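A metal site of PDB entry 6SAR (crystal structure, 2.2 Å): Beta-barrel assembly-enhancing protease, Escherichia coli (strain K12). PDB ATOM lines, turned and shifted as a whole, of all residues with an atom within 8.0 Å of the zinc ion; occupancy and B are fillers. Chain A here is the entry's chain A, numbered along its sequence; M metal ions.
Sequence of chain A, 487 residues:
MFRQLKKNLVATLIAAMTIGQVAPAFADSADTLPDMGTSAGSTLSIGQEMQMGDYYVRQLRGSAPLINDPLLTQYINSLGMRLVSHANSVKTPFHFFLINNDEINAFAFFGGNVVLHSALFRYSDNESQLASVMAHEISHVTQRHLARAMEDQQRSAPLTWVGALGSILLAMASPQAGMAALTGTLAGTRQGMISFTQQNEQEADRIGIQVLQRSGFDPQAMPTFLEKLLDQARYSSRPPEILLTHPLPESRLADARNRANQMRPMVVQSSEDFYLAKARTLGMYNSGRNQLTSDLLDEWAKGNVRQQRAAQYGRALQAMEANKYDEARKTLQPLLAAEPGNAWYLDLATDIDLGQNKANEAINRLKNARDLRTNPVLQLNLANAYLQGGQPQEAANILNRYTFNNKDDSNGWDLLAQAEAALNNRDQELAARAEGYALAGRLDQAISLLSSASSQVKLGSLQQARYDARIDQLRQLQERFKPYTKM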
ATOM      1  N   ALA A 106       8.207  19.371 -14.134  1.00  0.00           N
ATOM      2  CA  ALA A 106       7.911  18.392 -13.106  1.00  0.00           C
ATOM      3  C   ALA A 106       7.447  19.170 -11.892  1.00  0.00           C
ATOM      4  O   ALA A 106       7.941  20.260 -11.625  1.00  0.00           O
ATOM      5  CB  ALA A 106       9.152  17.583 -12.771  1.00  0.00           C
ATOM      6  N   VAL A 133      15.935  14.271 -11.987  1.00  0.00           N
ATOM      7  CA  VAL A 133      14.757  15.131 -11.897  1.00  0.00           C
ATOM      8  C   VAL A 133      13.732  14.565 -10.903  1.00  0.00           C
ATOM      9  O   VAL A 133      13.183  15.297 -10.091  1.00  0.00           O
ATOM     10  CB  VAL A 133      14.111  15.336 -13.286  1.00  0.00           C
ATOM     11  CG1 VAL A 133      12.841  16.162 -13.155  1.00  0.00           C
ATOM     12  CG2 VAL A 133      15.099  16.005 -14.229  1.00  0.00           C
ATOM     13  N   HIS A 136      15.123  15.094  -7.408  1.00  0.00           N
ATOM     14  CA  HIS A 136      14.932  16.494  -7.100  1.00  0.00           C
ATOM     15  C   HIS A 136      13.520  16.758  -6.562  1.00  0.00           C
ATOM     16  O   HIS A 136      13.345  17.411  -5.528  1.00  0.00           O
ATOM     17  CB  HIS A 136      15.207  17.297  -8.371  1.00  0.00           C
ATOM     18  CG  HIS A 136      15.074  18.774  -8.216  1.00  0.00           C
ATOM     19  ND1 HIS A 136      16.136  19.566  -7.853  1.00  0.00           N
ATOM     20  CD2 HIS A 136      14.034  19.599  -8.411  1.00  0.00           C
ATOM     21  CE1 HIS A 136      15.744  20.830  -7.812  1.00  0.00           C
ATOM     22  NE2 HIS A 136      14.470  20.871  -8.158  1.00  0.00           N
ATOM     23  N   GLU A 137      12.516  16.241  -7.263  1.00  0.00           N
ATOM     24  CA  GLU A 137      11.120  16.376  -6.833  1.00  0.00           C
ATOM     25  C   GLU A 137      10.837  15.704  -5.494  1.00  0.00           C
ATOM     26  O   GLU A 137      10.199  16.291  -4.619  1.00  0.00           O
ATOM     27  CB  GLU A 137      10.173  15.795  -7.893  1.00  0.00           C
ATOM     28  CG  GLU A 137      10.057  16.659  -9.140  1.00  0.00           C
ATOM     29  CD  GLU A 137       9.661  18.091  -8.802  1.00  0.00           C
ATOM     30  OE1 GLU A 137       8.637  18.280  -8.113  1.00  0.00           O
ATOM     31  OE2 GLU A 137      10.375  19.028  -9.228  1.00  0.00           O
ATOM     32  N   SER A 139      12.876  15.201  -3.191  1.00  0.00           N
ATOM     33  CA  SER A 139      13.524  16.010  -2.186  1.00  0.00           C
ATOM     34  C   SER A 139      12.727  17.275  -1.834  1.00  0.00           C
ATOM     35  O   SER A 139      12.691  17.683  -0.689  1.00  0.00           O
ATOM     36  CB  SER A 139      14.970  16.308  -2.594  1.00  0.00           C
ATOM     37  OG  SER A 139      15.674  15.079  -2.752  1.00  0.00           O
ATOM     38  N   HIS A 140      12.068  17.903  -2.820  1.00  0.00           N
ATOM     39  CA  HIS A 140      11.122  18.979  -2.495  1.00  0.00           C
ATOM     40  C   HIS A 140      10.063  18.478  -1.509  1.00  0.00           C
ATOM     41  O   HIS A 140       9.688  19.177  -0.574  1.00  0.00           O
ATOM     42  CB  HIS A 140      10.411  19.526  -3.726  1.00  0.00           C
ATOM     43  CG  HIS A 140      11.180  20.562  -4.470  1.00  0.00           C
ATOM     44  ND1 HIS A 140      11.519  21.776  -3.904  1.00  0.00           N
ATOM     45  CD2 HIS A 140      11.651  20.599  -5.734  1.00  0.00           C
ATOM     46  CE1 HIS A 140      12.166  22.507  -4.788  1.00  0.00           C
ATOM     47  NE2 HIS A 140      12.265  21.816  -5.906  1.00  0.00           N
ATOM     48  N   HIS A 145       8.925  21.645   1.122  1.00  0.00           N
ATOM     49  CA  HIS A 145       9.128  22.986   0.551  1.00  0.00           C
ATOM     50  C   HIS A 145       7.822  23.638   0.099  1.00  0.00           C
ATOM     51  O   HIS A 145       7.168  23.166  -0.822  1.00  0.00           O
ATOM     52  CB  HIS A 145      10.134  22.943  -0.606  1.00  0.00           C
ATOM     53  CG  HIS A 145      11.562  22.804  -0.155  1.00  0.00           C
ATOM     54  ND1 HIS A 145      12.532  22.181  -0.923  1.00  0.00           N
ATOM     55  CD2 HIS A 145      12.170  23.190   0.989  1.00  0.00           C
ATOM     56  CE1 HIS A 145      13.677  22.198  -0.274  1.00  0.00           C
ATOM     57  NE2 HIS A 145      13.483  22.804   0.889  1.00  0.00           N
ATOM     58  N   SER A 195       6.958  29.610  -8.071  1.00  0.00           N
ATOM     59  CA  SER A 195       8.255  28.943  -8.170  1.00  0.00           C
ATOM     60  C   SER A 195       8.984  28.872  -6.826  1.00  0.00           C
ATOM     61  O   SER A 195       8.547  29.484  -5.843  1.00  0.00           O
ATOM     62  CB  SER A 195       9.135  29.650  -9.214  1.00  0.00           C
ATOM     63  OG  SER A 195       9.690  30.844  -8.705  1.00  0.00           O
ATOM     64  N   PHE A 196      10.090  28.127  -6.779  1.00  0.00           N
ATOM     65  CA  PHE A 196      10.867  27.924  -5.541  1.00  0.00           C
ATOM     66  C   PHE A 196      12.032  28.909  -5.405  1.00  0.00           C
ATOM     67  O   PHE A 196      12.589  29.373  -6.398  1.00  0.00           O
ATOM     68  CB  PHE A 196      11.400  26.498  -5.469  1.00  0.00           C
ATOM     69  CG  PHE A 196      10.333  25.442  -5.423  1.00  0.00           C
ATOM     70  CD1 PHE A 196       9.767  25.044  -4.216  1.00  0.00           C
ATOM     71  CD2 PHE A 196       9.896  24.819  -6.595  1.00  0.00           C
ATOM     72  CE1 PHE A 196       8.799  24.052  -4.170  1.00  0.00           C
ATOM     73  CE2 PHE A 196       8.917  23.835  -6.554  1.00  0.00           C
ATOM     74  CZ  PHE A 196       8.366  23.452  -5.337  1.00  0.00           C
ATOM     75  N   THR A 197      12.396  29.204  -4.165  1.00  0.00           N
ATOM     76  CA  THR A 197      13.506  30.101  -3.855  1.00  0.00           C
ATOM     77  C   THR A 197      14.850  29.459  -4.195  1.00  0.00           C
ATOM     78  O   THR A 197      14.949  28.241  -4.357  1.00  0.00           O
ATOM     79  CB  THR A 197      13.590  30.430  -2.363  1.00  0.00           C
ATOM     80  OG1 THR A 197      13.866  29.231  -1.628  1.00  0.00           O
ATOM     81  CG2 THR A 197      12.303  31.073  -1.863  1.00  0.00           C
ATOM     82  N   ASN A 200      15.719  26.701  -1.611  1.00  0.00           N
ATOM     83  CA  ASN A 200      14.971  25.467  -1.826  1.00  0.00           C
ATOM     84  C   ASN A 200      15.545  24.653  -2.993  1.00  0.00           C
ATOM     85  O   ASN A 200      15.639  23.431  -2.913  1.00  0.00           O
ATOM     86  CB  ASN A 200      13.491  25.757  -2.127  1.00  0.00           C
ATOM     87  CG  ASN A 200      12.733  26.321  -0.934  1.00  0.00           C
ATOM     88  OD1 ASN A 200      13.081  26.079   0.222  1.00  0.00           O
ATOM     89  ND2 ASN A 200      11.695  27.095  -1.223  1.00  0.00           N
ATOM     90  N   GLU A 201      15.907  25.330  -4.083  1.00  0.00           N
ATOM     91  CA  GLU A 201      16.497  24.664  -5.235  1.00  0.00           C
ATOM     92  C   GLU A 201      17.844  24.023  -4.895  1.00  0.00           C
ATOM     93  O   GLU A 201      18.092  22.885  -5.277  1.00  0.00           O
ATOM     94  CB  GLU A 201      16.621  25.624  -6.412  1.00  0.00           C
ATOM     95  CG  GLU A 201      15.273  26.021  -6.983  1.00  0.00           C
ATOM     96  CD  GLU A 201      14.465  24.796  -7.381  1.00  0.00           C
ATOM     97  OE1 GLU A 201      14.978  23.972  -8.144  1.00  0.00           O
ATOM     98  OE2 GLU A 201      13.329  24.653  -6.909  1.00  0.00           O
ATOM     99  N   GLN A 202      18.690  24.759  -4.185  1.00  0.00           N
ATOM    100  CA  GLN A 202      19.984  24.249  -3.754  1.00  0.00           C
ATOM    101  C   GLN A 202      19.810  23.023  -2.856  1.00  0.00           C
ATOM    102  O   GLN A 202      20.449  22.006  -3.072  1.00  0.00           O
ATOM    103  CB  GLN A 202      20.760  25.338  -3.021  1.00  0.00           C
ATOM    104  CG  GLN A 202      22.201  24.978  -2.725  1.00  0.00           C
ATOM    105  CD  GLN A 202      23.002  26.179  -2.255  1.00  0.00           C
ATOM    106  OE1 GLN A 202      23.296  27.083  -3.038  1.00  0.00           O
ATOM    107  NE2 GLN A 202      23.344  26.202  -0.981  1.00  0.00           N
ATOM    108  N   ALA A 204      17.228  20.957  -2.645  1.00  0.00           N
ATOM    109  CA  ALA A 204      16.656  19.845  -3.385  1.00  0.00           C
ATOM    110  C   ALA A 204      17.702  19.129  -4.263  1.00  0.00           C
ATOM    111  O   ALA A 204      17.664  17.909  -4.422  1.00  0.00           O
ATOM    112  CB  ALA A 204      15.476  20.315  -4.212  1.00  0.00           C
ATOM    113  N   ASP A 205      18.619  19.920  -4.823  1.00  0.00           N
ATOM    114  CA  ASP A 205      19.767  19.401  -5.584  1.00  0.00           C
ATOM    115  C   ASP A 205      20.723  18.599  -4.703  1.00  0.00           C
ATOM    116  O   ASP A 205      21.169  17.518  -5.097  1.00  0.00           O
ATOM    117  CB  ASP A 205      20.536  20.539  -6.260  1.00  0.00           C
ATOM    118  CG  ASP A 205      19.866  21.045  -7.533  1.00  0.00           C
ATOM    119  OD1 ASP A 205      18.935  20.389  -8.062  1.00  0.00           O
ATOM    120  OD2 ASP A 205      20.302  22.122  -8.016  1.00  0.00           O
ATOM    121  N   ILE A 242      10.299  24.330 -17.135  1.00  0.00           N
ATOM    122  CA  ILE A 242      10.787  23.853 -15.855  1.00  0.00           C
ATOM    123  C   ILE A 242      11.654  24.871 -15.111  1.00  0.00           C
ATOM    124  O   ILE A 242      11.663  24.898 -13.881  1.00  0.00           O
ATOM    125  CB  ILE A 242      11.554  22.516 -16.019  1.00  0.00           C
ATOM    126  CG1 ILE A 242      11.756  21.836 -14.664  1.00  0.00           C
ATOM    127  CG2 ILE A 242      12.905  22.733 -16.704  1.00  0.00           C
ATOM    128  CD1 ILE A 242      12.356  20.449 -14.768  1.00  0.00           C
ATOM    129  N   THR A 245       9.667  27.350 -12.953  1.00  0.00           N
ATOM    130  CA  THR A 245       9.238  26.748 -11.696  1.00  0.00           C
ATOM    131  C   THR A 245      10.415  26.449 -10.760  1.00  0.00           C
ATOM    132  O   THR A 245      10.313  26.634  -9.540  1.00  0.00           O
ATOM    133  CB  THR A 245       8.502  25.436 -12.015  1.00  0.00           C
ATOM    134  OG1 THR A 245       7.607  25.660 -13.118  1.00  0.00           O
ATOM    135  CG2 THR A 245       7.742  24.910 -10.815  1.00  0.00           C
ATOM    136  N   HIS A 246      11.519  25.969 -11.336  1.00  0.00           N
ATOM    137  CA  HIS A 246      12.740  25.612 -10.620  1.00  0.00           C
ATOM    138  C   HIS A 246      13.905  26.422 -11.185  1.00  0.00           C
ATOM    139  O   HIS A 246      14.645  25.931 -12.055  1.00  0.00           O
ATOM    140  CB  HIS A 246      13.032  24.122 -10.837  1.00  0.00           C
ATOM    141  CG  HIS A 246      11.913  23.224 -10.439  1.00  0.00           C
ATOM    142  ND1 HIS A 246      11.758  22.727  -9.163  1.00  0.00           N
ATOM    143  CD2 HIS A 246      10.852  22.755 -11.139  1.00  0.00           C
ATOM    144  CE1 HIS A 246      10.667  21.984  -9.100  1.00  0.00           C
ATOM    145  NE2 HIS A 246      10.094  21.987 -10.290  1.00  0.00           N
ATOM    146  N   PRO A 247      14.079  27.669 -10.714  1.00  0.00           N
ATOM    147  CA  PRO A 247      15.070  28.551 -11.351  1.00  0.00           C
ATOM    148  C   PRO A 247      16.464  27.967 -11.338  1.00  0.00           C
ATOM    149  O   PRO A 247      16.850  27.285 -10.376  1.00  0.00           O
ATOM    150  CB  PRO A 247      15.011  29.831 -10.496  1.00  0.00           C
ATOM    151  CG  PRO A 247      13.697  29.786  -9.806  1.00  0.00           C
ATOM    152  CD  PRO A 247      13.375  28.330  -9.605  1.00  0.00           C
ATOM    153  N   ARG A 252      23.768  27.681  -9.221  1.00  0.00           N
ATOM    154  CA  ARG A 252      23.126  26.414  -8.969  1.00  0.00           C
ATOM    155  C   ARG A 252      23.773  25.294  -9.773  1.00  0.00           C
ATOM    156  O   ARG A 252      23.981  24.195  -9.246  1.00  0.00           O
ATOM    157  CB  ARG A 252      21.610  26.490  -9.258  1.00  0.00           C
ATOM    158  CG  ARG A 252      20.835  25.271  -8.784  1.00  0.00           C
ATOM    159  CD  ARG A 252      19.358  25.315  -9.137  1.00  0.00           C
ATOM    160  NE  ARG A 252      18.849  23.952  -9.246  1.00  0.00           N
ATOM    161  CZ  ARG A 252      17.821  23.553  -9.999  1.00  0.00           C
ATOM    162  NH1 ARG A 252      17.115  24.413 -10.722  1.00  0.00           N
ATOM    163  NH2 ARG A 252      17.511  22.267 -10.016  1.00  0.00           N
HETATM  164 ZN    ZN M   1      13.097  22.491  -7.732  1.00  0.00          ZN
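The zinc ion is bound by ND1 of His 246 (2.0 Å), NE2 of His 140 (2.1 Å), NE2 of His 136 (2.2 Å), OE2 of Glu 201 (2.3 Å) and OE1 of Glu 201 (2.4 Å).
A ring nitrogen (NE2) of His 246 sits close to the side-chain carboxylate of Glu 137, at 3.2 Å. The backbone carbonyl oxygen (O) of His 246 lies within hydrogen-bond range of the guanidinium group (NH1) of Arg 252, at 3.2 Å. The backbone carbonyl oxygen of Ala 106 lies within hydrogen-bond range of a ring nitrogen (NE2) of His 246 (3.1 Å). The backbone carbonyl oxygen of His 140 sits at hydrogen-bond distance from the backbone NH of His 145, at 3.1 Å. The side-chain carboxylate of Asp 205 sits at hydrogen-bond distance from a ring nitrogen (ND1) of His 136, at 2.9 Å. The side-chain carboxylate of Glu 201 lies close to the guanidinium group of Arg 252.
Four residues have an atom within 4 Å of the zinc ion: His 136, His 140, Glu 201 and His 246. The nearest printed residue that does not touch the zinc ion is Phe 196 (4.1 Å).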
